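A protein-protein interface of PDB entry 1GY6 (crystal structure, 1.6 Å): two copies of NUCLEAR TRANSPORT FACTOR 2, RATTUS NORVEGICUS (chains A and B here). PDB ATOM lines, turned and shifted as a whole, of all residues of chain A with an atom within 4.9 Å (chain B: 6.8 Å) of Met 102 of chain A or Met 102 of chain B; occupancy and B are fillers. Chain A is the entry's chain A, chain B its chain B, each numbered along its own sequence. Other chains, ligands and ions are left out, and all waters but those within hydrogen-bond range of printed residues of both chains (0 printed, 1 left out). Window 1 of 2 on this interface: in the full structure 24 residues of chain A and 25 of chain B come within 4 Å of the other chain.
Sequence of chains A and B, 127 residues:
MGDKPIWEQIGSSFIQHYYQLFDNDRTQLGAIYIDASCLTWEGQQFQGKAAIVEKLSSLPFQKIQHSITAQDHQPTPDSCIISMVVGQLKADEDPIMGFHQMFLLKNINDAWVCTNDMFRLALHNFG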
ATOM      1  N   ILE A  82      17.067  -7.778   4.096  1.00  0.00           N
ATOM      2  CA  ILE A  82      16.359  -8.601   5.065  1.00  0.00           C
ATOM      3  C   ILE A  82      17.204  -9.831   5.300  1.00  0.00           C
ATOM      4  O   ILE A  82      17.807 -10.381   4.373  1.00  0.00           O
ATOM      5  CB  ILE A  82      14.922  -8.929   4.584  1.00  0.00           C
ATOM      6  CG1 ILE A  82      14.126  -9.565   5.723  1.00  0.00           C
ATOM      7  CG2 ILE A  82      14.953  -9.787   3.339  1.00  0.00           C
ATOM      8  CD1 ILE A  82      12.624  -9.420   5.496  1.00  0.00           C
ATOM      9  N   SER A  83      17.280 -10.245   6.555  1.00  0.00           N
ATOM     10  CA  SER A  83      18.145 -11.358   6.922  1.00  0.00           C
ATOM     11  C   SER A  83      17.464 -12.335   7.844  1.00  0.00           C
ATOM     12  O   SER A  83      16.756 -11.928   8.756  1.00  0.00           O
ATOM     13  CB  SER A  83      19.380 -10.828   7.649  1.00  0.00           C
ATOM     14  OG  SER A  83      20.066  -9.843   6.892  1.00  0.00           O
ATOM     15  N   MET A  84      17.670 -13.624   7.598  1.00  0.00           N
ATOM     16  CA  MET A  84      17.118 -14.642   8.487  1.00  0.00           C
ATOM     17  C   MET A  84      18.278 -15.436   9.086  1.00  0.00           C
ATOM     18  O   MET A  84      19.181 -15.873   8.366  1.00  0.00           O
ATOM     19  CB  MET A  84      16.162 -15.574   7.728  1.00  0.00           C
ATOM     20  CG  MET A  84      15.495 -16.586   8.622  1.00  0.00           C
ATOM     21  SD  MET A  84      14.123 -17.478   7.838  1.00  0.00           S
ATOM     22  CE  MET A  84      15.009 -18.800   7.158  1.00  0.00           C
ATOM     23  N   HIS A 100      15.588 -18.573  16.208  1.00  0.00           N
ATOM     24  CA  HIS A 100      15.408 -18.041  14.868  1.00  0.00           C
ATOM     25  C   HIS A 100      15.337 -16.536  15.049  1.00  0.00           C
ATOM     26  O   HIS A 100      14.741 -16.076  15.995  1.00  0.00           O
ATOM     27  CB  HIS A 100      14.112 -18.560  14.216  1.00  0.00           C
ATOM     28  CG  HIS A 100      13.832 -17.933  12.881  1.00  0.00           C
ATOM     29  ND1 HIS A 100      13.502 -18.664  11.761  1.00  0.00           N
ATOM     30  CD2 HIS A 100      13.766 -16.632  12.505  1.00  0.00           C
ATOM     31  CE1 HIS A 100      13.231 -17.848  10.760  1.00  0.00           C
ATOM     32  NE2 HIS A 100      13.383 -16.605  11.185  1.00  0.00           N
ATOM     33  N   GLN A 101      15.957 -15.767  14.161  1.00  0.00           N
ATOM     34  CA  GLN A 101      15.875 -14.301  14.302  1.00  0.00           C
ATOM     35  C   GLN A 101      15.841 -13.673  12.931  1.00  0.00           C
ATOM     36  O   GLN A 101      16.456 -14.178  12.019  1.00  0.00           O
ATOM     37  CB  GLN A 101      17.086 -13.799  15.091  1.00  0.00           C
ATOM     38  CG  GLN A 101      17.107 -12.309  15.399  1.00  0.00           C
ATOM     39  CD  GLN A 101      17.863 -11.974  16.687  1.00  0.00           C
ATOM     40  OE1 GLN A 101      18.742 -12.710  17.118  1.00  0.00           O
ATOM     41  NE2 GLN A 101      17.489 -10.870  17.315  1.00  0.00           N
ATOM     42  N   MET A 102      15.112 -12.575  12.795  1.00  0.00           N
ATOM     43  CA  MET A 102      15.037 -11.870  11.517  1.00  0.00           C
ATOM     44  C   MET A 102      15.463 -10.421  11.747  1.00  0.00           C
ATOM     45  O   MET A 102      15.179  -9.854  12.791  1.00  0.00           O
ATOM     46  CB  MET A 102      13.597 -11.901  10.962  1.00  0.00           C
ATOM     47  CG  MET A 102      13.387 -11.107   9.633  1.00  0.00           C
ATOM     48  SD  MET A 102      13.406  -9.251   9.853  1.00  0.00           S
ATOM     49  CE  MET A 102      12.559  -9.124  11.246  1.00  0.00           C
ATOM     50  N   PHE A 103      16.203  -9.855  10.795  1.00  0.00           N
ATOM     51  CA  PHE A 103      16.569  -8.425  10.848  1.00  0.00           C
ATOM     52  C   PHE A 103      16.235  -7.724   9.538  1.00  0.00           C
ATOM     53  O   PHE A 103      16.432  -8.298   8.450  1.00  0.00           O
ATOM     54  CB  PHE A 103      18.077  -8.228  11.067  1.00  0.00           C
ATOM     55  CG  PHE A 103      18.610  -8.874  12.316  1.00  0.00           C
ATOM     56  CD1 PHE A 103      19.266 -10.103  12.253  1.00  0.00           C
ATOM     57  CD2 PHE A 103      18.502  -8.231  13.545  1.00  0.00           C
ATOM     58  CE1 PHE A 103      19.826 -10.669  13.405  1.00  0.00           C
ATOM     59  CE2 PHE A 103      19.069  -8.803  14.716  1.00  0.00           C
ATOM     60  CZ  PHE A 103      19.726 -10.012  14.631  1.00  0.00           C
ATOM     61  N   LEU A 104      15.707  -6.505   9.631  1.00  0.00           N
ATOM     62  CA  LEU A 104      15.488  -5.687   8.417  1.00  0.00           C
ATOM     63  C   LEU A 104      16.408  -4.485   8.597  1.00  0.00           C
ATOM     64  O   LEU A 104      16.330  -3.775   9.614  1.00  0.00           O
ATOM     65  CB  LEU A 104      14.044  -5.233   8.291  1.00  0.00           C
ATOM     66  CG  LEU A 104      13.742  -4.440   7.018  1.00  0.00           C
ATOM     67  CD1 LEU A 104      14.035  -5.301   5.768  1.00  0.00           C
ATOM     68  CD2 LEU A 104      12.293  -3.992   7.052  1.00  0.00           C
ATOM     69  N   ASN A 116      13.734  -3.450  12.151  1.00  0.00           N
ATOM     70  CA  ASN A 116      12.841  -4.512  12.623  1.00  0.00           C
ATOM     71  C   ASN A 116      13.702  -5.682  13.034  1.00  0.00           C
ATOM     72  O   ASN A 116      14.585  -6.091  12.279  1.00  0.00           O
ATOM     73  CB  ASN A 116      11.930  -4.924  11.463  1.00  0.00           C
ATOM     74  CG  ASN A 116      10.882  -3.902  11.164  1.00  0.00           C
ATOM     75  OD1 ASN A 116       9.737  -4.006  11.685  1.00  0.00           O
ATOM     76  ND2 ASN A 116      11.218  -2.925  10.349  1.00  0.00           N
ATOM     77  N   ASP A 117      13.454  -6.193  14.231  1.00  0.00           N
ATOM     78  CA  ASP A 117      14.215  -7.326  14.812  1.00  0.00           C
ATOM     79  C   ASP A 117      13.169  -8.252  15.440  1.00  0.00           C
ATOM     80  O   ASP A 117      12.346  -7.792  16.236  1.00  0.00           O
ATOM     81  CB  ASP A 117      15.168  -6.746  15.875  1.00  0.00           C
ATOM     82  CG  ASP A 117      15.975  -7.793  16.624  1.00  0.00           C
ATOM     83  OD1 ASP A 117      15.711  -9.006  16.456  1.00  0.00           O
ATOM     84  OD2 ASP A 117      16.886  -7.362  17.410  1.00  0.00           O
ATOM     85  N   MET A 118      13.131  -9.518  15.018  1.00  0.00           N
ATOM     86  CA  MET A 118      12.177 -10.500  15.582  1.00  0.00           C
ATOM     87  C   MET A 118      12.969 -11.709  16.055  1.00  0.00           C
ATOM     88  O   MET A 118      13.733 -12.270  15.288  1.00  0.00           O
ATOM     89  CB  MET A 118      11.170 -10.916  14.505  1.00  0.00           C
ATOM     90  CG  MET A 118      10.464  -9.692  13.962  1.00  0.00           C
ATOM     91  SD  MET A 118       9.346 -10.034  12.585  1.00  0.00           S
ATOM     92  CE  MET A 118       8.123 -10.650  13.678  1.00  0.00           C
ATOM     93  N   TYR B  19       0.214 -21.545   3.080  1.00  0.00           N
ATOM     94  CA  TYR B  19       0.273 -22.961   3.425  1.00  0.00           C
ATOM     95  C   TYR B  19      -0.913 -23.743   2.871  1.00  0.00           C
ATOM     96  O   TYR B  19      -0.768 -24.917   2.551  1.00  0.00           O
ATOM     97  CB  TYR B  19       0.468 -23.163   4.940  1.00  0.00           C
ATOM     98  CG  TYR B  19       1.849 -22.695   5.385  1.00  0.00           C
ATOM     99  CD1 TYR B  19       1.999 -21.549   6.167  1.00  0.00           C
ATOM    100  CD2 TYR B  19       3.004 -23.370   4.956  1.00  0.00           C
ATOM    101  CE1 TYR B  19       3.235 -21.072   6.513  1.00  0.00           C
ATOM    102  CE2 TYR B  19       4.272 -22.901   5.301  1.00  0.00           C
ATOM    103  CZ  TYR B  19       4.372 -21.754   6.070  1.00  0.00           C
ATOM    104  OH  TYR B  19       5.592 -21.213   6.377  1.00  0.00           O
ATOM    105  N   GLN B  74       5.296  -8.283  12.160  1.00  0.00           N
ATOM    106  CA  GLN B  74       5.619  -6.881  12.461  1.00  0.00           C
ATOM    107  C   GLN B  74       5.408  -5.985  11.259  1.00  0.00           C
ATOM    108  O   GLN B  74       5.616  -6.399  10.126  1.00  0.00           O
ATOM    109  CB  GLN B  74       7.093  -6.667  12.754  1.00  0.00           C
ATOM    110  CG  GLN B  74       7.552  -7.079  14.077  1.00  0.00           C
ATOM    111  CD  GLN B  74       8.994  -6.634  14.316  1.00  0.00           C
ATOM    112  OE1 GLN B  74       9.702  -6.200  13.391  1.00  0.00           O
ATOM    113  NE2 GLN B  74       9.446  -6.772  15.547  1.00  0.00           N
ATOM    114  N   ILE B  82       6.487  -8.090   8.010  1.00  0.00           N
ATOM    115  CA  ILE B  82       7.402  -9.242   8.076  1.00  0.00           C
ATOM    116  C   ILE B  82       6.685 -10.315   8.885  1.00  0.00           C
ATOM    117  O   ILE B  82       6.164 -10.019   9.966  1.00  0.00           O
ATOM    118  CB  ILE B  82       8.700  -8.893   8.845  1.00  0.00           C
ATOM    119  CG1 ILE B  82       9.400  -7.724   8.179  1.00  0.00           C
ATOM    120  CG2 ILE B  82       9.612 -10.144   8.934  1.00  0.00           C
ATOM    121  CD1 ILE B  82      10.399  -7.068   9.093  1.00  0.00           C
ATOM    122  N   SER B  83       6.699 -11.564   8.404  1.00  0.00           N
ATOM    123  CA  SER B  83       6.064 -12.685   9.104  1.00  0.00           C
ATOM    124  C   SER B  83       7.137 -13.742   9.326  1.00  0.00           C
ATOM    125  O   SER B  83       7.838 -14.117   8.389  1.00  0.00           O
ATOM    126  CB  SER B  83       4.936 -13.256   8.251  1.00  0.00           C
ATOM    127  OG  SER B  83       3.892 -12.284   8.024  1.00  0.00           O
ATOM    128  N   MET B  84       7.270 -14.199  10.569  1.00  0.00           N
ATOM    129  CA  MET B  84       8.306 -15.188  10.916  1.00  0.00           C
ATOM    130  C   MET B  84       7.585 -16.399  11.453  1.00  0.00           C
ATOM    131  O   MET B  84       6.844 -16.280  12.421  1.00  0.00           O
ATOM    132  CB  MET B  84       9.230 -14.591  11.984  1.00  0.00           C
ATOM    133  CG  MET B  84      10.420 -15.496  12.311  1.00  0.00           C
ATOM    134  SD  MET B  84      11.690 -14.632  13.299  1.00  0.00           S
ATOM    135  CE  MET B  84      11.022 -14.900  14.966  1.00  0.00           C
ATOM    136  N   VAL B  85       7.837 -17.559  10.852  1.00  0.00           N
ATOM    137  CA  VAL B  85       7.124 -18.783  11.202  1.00  0.00           C
ATOM    138  C   VAL B  85       8.020 -19.931  11.608  1.00  0.00           C
ATOM    139  O   VAL B  85       9.090 -20.075  11.046  1.00  0.00           O
ATOM    140  CB  VAL B  85       6.325 -19.230   9.944  1.00  0.00           C
ATOM    141  CG1 VAL B  85       5.569 -20.536  10.192  1.00  0.00           C
ATOM    142  CG2 VAL B  85       5.392 -18.090   9.530  1.00  0.00           C
ATOM    143  N   HIS B 100      11.678 -23.473   9.514  1.00  0.00           N
ATOM    144  CA  HIS B 100      11.632 -22.054   9.813  1.00  0.00           C
ATOM    145  C   HIS B 100      11.397 -21.329   8.484  1.00  0.00           C
ATOM    146  O   HIS B 100      12.019 -21.653   7.469  1.00  0.00           O
ATOM    147  CB  HIS B 100      12.963 -21.564  10.373  1.00  0.00           C
ATOM    148  CG  HIS B 100      13.319 -22.171  11.689  1.00  0.00           C
ATOM    149  ND1 HIS B 100      12.713 -21.807  12.875  1.00  0.00           N
ATOM    150  CD2 HIS B 100      14.166 -23.182  11.989  1.00  0.00           C
ATOM    151  CE1 HIS B 100      13.168 -22.575  13.851  1.00  0.00           C
ATOM    152  NE2 HIS B 100      14.047 -23.417  13.336  1.00  0.00           N
ATOM    153  N   GLN B 101      10.529 -20.324   8.485  1.00  0.00           N
ATOM    154  CA  GLN B 101      10.290 -19.596   7.259  1.00  0.00           C
ATOM    155  C   GLN B 101      10.010 -18.140   7.581  1.00  0.00           C
ATOM    156  O   GLN B 101       9.466 -17.824   8.650  1.00  0.00           O
ATOM    157  CB  GLN B 101       9.126 -20.257   6.486  1.00  0.00           C
ATOM    158  CG  GLN B 101       8.916 -19.695   5.084  1.00  0.00           C
ATOM    159  CD  GLN B 101       8.263 -20.680   4.153  1.00  0.00           C
ATOM    160  OE1 GLN B 101       7.569 -21.599   4.582  1.00  0.00           O
ATOM    161  NE2 GLN B 101       8.445 -20.471   2.835  1.00  0.00           N
ATOM    162  N   MET B 102      10.402 -17.243   6.680  1.00  0.00           N
ATOM    163  CA  MET B 102      10.177 -15.805   6.899  1.00  0.00           C
ATOM    164  C   MET B 102       9.638 -15.216   5.607  1.00  0.00           C
ATOM    165  O   MET B 102      10.055 -15.634   4.509  1.00  0.00           O
ATOM    166  CB  MET B 102      11.519 -15.142   7.295  1.00  0.00           C
ATOM    167  CG  MET B 102      11.467 -13.676   7.778  1.00  0.00           C
ATOM    168  SD  MET B 102      12.612 -12.696   6.810  1.00  0.00           S
ATOM    169  CE  MET B 102      11.457 -12.749   5.388  1.00  0.00           C
ATOM    170  N   PHE B 103       8.693 -14.284   5.710  1.00  0.00           N
ATOM    171  CA  PHE B 103       8.136 -13.666   4.507  1.00  0.00           C
ATOM    172  C   PHE B 103       8.104 -12.161   4.664  1.00  0.00           C
ATOM    173  O   PHE B 103       7.815 -11.668   5.742  1.00  0.00           O
ATOM    174  CB  PHE B 103       6.671 -14.094   4.277  1.00  0.00           C
ATOM    175  CG  PHE B 103       6.444 -15.580   4.240  1.00  0.00           C
ATOM    176  CD1 PHE B 103       6.030 -16.256   5.387  1.00  0.00           C
ATOM    177  CD2 PHE B 103       6.568 -16.300   3.035  1.00  0.00           C
ATOM    178  CE1 PHE B 103       5.718 -17.650   5.334  1.00  0.00           C
ATOM    179  CE2 PHE B 103       6.274 -17.657   2.968  1.00  0.00           C
ATOM    180  CZ  PHE B 103       5.845 -18.335   4.112  1.00  0.00           C
ATOM    181  N   LEU B 104       8.397 -11.436   3.583  1.00  0.00           N
ATOM    182  CA  LEU B 104       8.248  -9.985   3.617  1.00  0.00           C
ATOM    183  C   LEU B 104       7.099  -9.728   2.647  1.00  0.00           C
ATOM    184  O   LEU B 104       7.119 -10.209   1.499  1.00  0.00           O
ATOM    185  CB  LEU B 104       9.520  -9.268   3.147  1.00  0.00           C
ATOM    186  CG  LEU B 104       9.400  -7.742   3.168  1.00  0.00           C
ATOM    187  CD1 LEU B 104       9.258  -7.211   4.591  1.00  0.00           C
ATOM    188  CD2 LEU B 104      10.662  -7.172   2.516  1.00  0.00           C
ATOM    189  N   CYS B 114       3.846 -11.469  -1.416  1.00  0.00           N
ATOM    190  CA  CYS B 114       5.169 -11.729  -0.876  1.00  0.00           C
ATOM    191  C   CYS B 114       6.292 -11.344  -1.848  1.00  0.00           C
ATOM    192  O   CYS B 114       6.309 -11.826  -3.010  1.00  0.00           O
ATOM    193  CB  CYS B 114       5.271 -13.207  -0.539  1.00  0.00           C
ATOM    194  SG  CYS B 114       6.923 -13.679   0.046  1.00  0.00           S
ATOM    195  N   ASN B 116       9.684 -11.338  -0.683  1.00  0.00           N
ATOM    196  CA  ASN B 116      10.880 -12.036  -0.220  1.00  0.00           C
ATOM    197  C   ASN B 116      10.437 -13.182   0.671  1.00  0.00           C
ATOM    198  O   ASN B 116       9.573 -13.017   1.528  1.00  0.00           O
ATOM    199  CB  ASN B 116      11.750 -11.078   0.599  1.00  0.00           C
ATOM    200  CG  ASN B 116      12.335  -9.963  -0.222  1.00  0.00           C
ATOM    201  OD1 ASN B 116      13.486 -10.048  -0.668  1.00  0.00           O
ATOM    202  ND2 ASN B 116      11.582  -8.904  -0.411  1.00  0.00           N
ATOM    203  N   ASP B 117      11.051 -14.351   0.457  1.00  0.00           N
ATOM    204  CA  ASP B 117      10.717 -15.582   1.181  1.00  0.00           C
ATOM    205  C   ASP B 117      12.017 -16.338   1.464  1.00  0.00           C
ATOM    206  O   ASP B 117      12.848 -16.486   0.558  1.00  0.00           O
ATOM    207  CB  ASP B 117       9.789 -16.370   0.242  1.00  0.00           C
ATOM    208  CG  ASP B 117       9.318 -17.732   0.775  1.00  0.00           C
ATOM    209  OD1 ASP B 117       9.826 -18.194   1.811  1.00  0.00           O
ATOM    210  OD2 ASP B 117       8.438 -18.361   0.107  1.00  0.00           O
ATOM    211  N   MET B 118      12.203 -16.780   2.717  1.00  0.00           N
ATOM    212  CA  MET B 118      13.379 -17.585   3.082  1.00  0.00           C
ATOM    213  C   MET B 118      12.889 -18.801   3.864  1.00  0.00           C
ATOM    214  O   MET B 118      12.130 -18.669   4.820  1.00  0.00           O
ATOM    215  CB  MET B 118      14.356 -16.779   3.937  1.00  0.00           C
ATOM    216  CG  MET B 118      14.977 -15.618   3.171  1.00  0.00           C
ATOM    217  SD  MET B 118      15.985 -14.561   4.282  1.00  0.00           S
ATOM    218  CE  MET B 118      16.768 -13.513   3.121  1.00  0.00           C
ATOM    219  N   PHE B 119      13.351 -19.974   3.460  1.00  0.00           N
ATOM    220  CA  PHE B 119      12.921 -21.229   4.092  1.00  0.00           C
ATOM    221  C   PHE B 119      14.106 -22.127   4.451  1.00  0.00           C
ATOM    222  O   PHE B 119      15.023 -22.294   3.645  1.00  0.00           O
ATOM    223  CB  PHE B 119      12.017 -21.995   3.117  1.00  0.00           C
ATOM    224  CG  PHE B 119      11.676 -23.383   3.575  1.00  0.00           C
ATOM    225  CD1 PHE B 119      10.573 -23.618   4.395  1.00  0.00           C
ATOM    226  CD2 PHE B 119      12.471 -24.466   3.191  1.00  0.00           C
ATOM    227  CE1 PHE B 119      10.273 -24.914   4.805  1.00  0.00           C
ATOM    228  CE2 PHE B 119      12.167 -25.758   3.605  1.00  0.00           C
ATOM    229  CZ  PHE B 119      11.051 -25.970   4.423  1.00  0.00           C
ATOM    230  N   ARG B 120      14.047 -22.747   5.625  1.00  0.00           N
ATOM    231  CA  ARG B 120      15.112 -23.655   6.092  1.00  0.00           C
ATOM    232  C   ARG B 120      14.491 -24.820   6.849  1.00  0.00           C
ATOM    233  O   ARG B 120      13.654 -24.621   7.702  1.00  0.00           O
ATOM    234  CB  ARG B 120      16.075 -22.933   7.062  1.00  0.00           C
ATOM    235  CG  ARG B 120      17.029 -21.890   6.452  1.00  0.00           C
ATOM    236  CD  ARG B 120      18.394 -22.468   6.272  1.00  0.00           C
ATOM    237  NE  ARG B 120      19.300 -21.612   5.515  1.00  0.00           N
ATOM    238  CZ  ARG B 120      20.408 -22.059   4.934  1.00  0.00           C
ATOM    239  NH1 ARG B 120      20.731 -23.342   5.040  1.00  0.00           N
ATOM    240  NH2 ARG B 120      21.177 -21.235   4.244  1.00  0.00           N
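ND1 of His 100 of chain A lies close to ND1 of His 100 of chain B, 3.4 Å away. O of Asp 117 of chain A is in hydrogen-bond range of NE2 of Gln 74 of chain B (3.2 Å). OE1 of Gln 74 of chain B sits close to OD1 of Asn 116 of chain A (2.8 Å). The backbone carbonyl oxygen of Met 118 of chain A lies close to the side-chain sulfur of Met 84 of chain B. NE2 of His 100 of chain A lies close to SD of Met 84 of chain B (3.4 Å).
SD of Met 102 of chain A lies within hydrogen-bond range of N of Leu 104 of chain A, at 3.6 Å. N of Leu 104 of chain B lies within hydrogen-bond range of O of Asn 116 of chain B (2.8 Å). SG of Cys 114 of chain B lies close to O of Leu 104 of chain B, 3.8 Å away. The side-chain sulfur of Met 84 of chain A lies close to a ring nitrogen (NE2) of His 100 of chain A (3.5 Å). N of Leu 104 of chain A is in hydrogen-bond range of O of Asn 116 of chain A, at 2.9 Å. The backbone carbonyl oxygen (O) of Gln 74 of chain B is in hydrogen-bond range of the backbone NH (N) of Ile 82 of chain B (2.8 Å).
Ile 82 of chain A touches Met 102 of chain B. CD1 of Ile 82 of chain A touches CB of Leu 104 of chain B, 3.9 Å away. Ile 82 of chain A touches Met 118 of chain B. Met 84 of chain A touches Met 102 of chain B. SD of Met 118 of chain B touches CB of Met 84 of chain A, at 3.6 Å. Met 102 of chain A touches Ile 82 of chain B (CE to CD1, 3.7 Å). CG of Met 102 of chain A touches SD of Met 102 of chain B, at 3.3 Å. Asn 116 of chain A touches Ile 82 of chain B (CB to CD1, 3.5 Å). Met 118 of chain A touches Gln 74 of chain B. SD of Met 118 of chain A touches CG2 of Ile 82 of chain B, 3.7 Å away.
Of the printed residues of chain B, His 100 of chain A touches Met 84 (3.0 Å) and His 100 (3.3 Å). Met 102 of chain A touches just these residues of chain B: Ile 82 (3.7 Å) and Met 102 (3.3 Å). Of the printed residues of chain B, Asp 117 of chain A touches Gln 74. Of the printed residues of chain A, Ile 82 of chain B touches Met 102, Asn 116 and Met 118. Of the printed residues of chain A, Met 84 of chain B touches His 100 (3.0 Å) and Met 118 (3.7 Å). Of the printed residues of chain A, Met 102 of chain B touches Ile 82 (3.5 Å), Met 84 (3.5 Å) and Met 102 (3.3 Å). Of the printed residues of chain A, Met 118 of chain B touches Ile 82 and Met 84.
Along chain B the printed residues that touch a printed residue of chain A span positions 74 to 120. Along chain A the printed residues that touch a printed residue of chain B span positions 82 to 118. Among the printed residues, no Asp or Glu carboxylate lies within 4 Å of a Lys or Arg side-chain nitrogen of the other chain.
Ile 82 of chain A touches Met 118 of chain B, and with the chains exchanged Met 118 of chain A touches Ile 82 of chain B. His 100 of chain A touches Met 84 of chain B, but with the chains exchanged Met 84 of chain A does not touch His 100 of chain B (4.1 Å). His 100 of chain A touches its own counterpart, His 100 of chain B. Asn 116 of chain A touches Ile 82 of chain B, but with the chains exchanged Ile 82 of chain A does not touch Asn 116 of chain B (4.3 Å). Positions printed for both chains: 82, 83, 84, 100, 101, 102, 103, 104, 116, 117 and 118.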
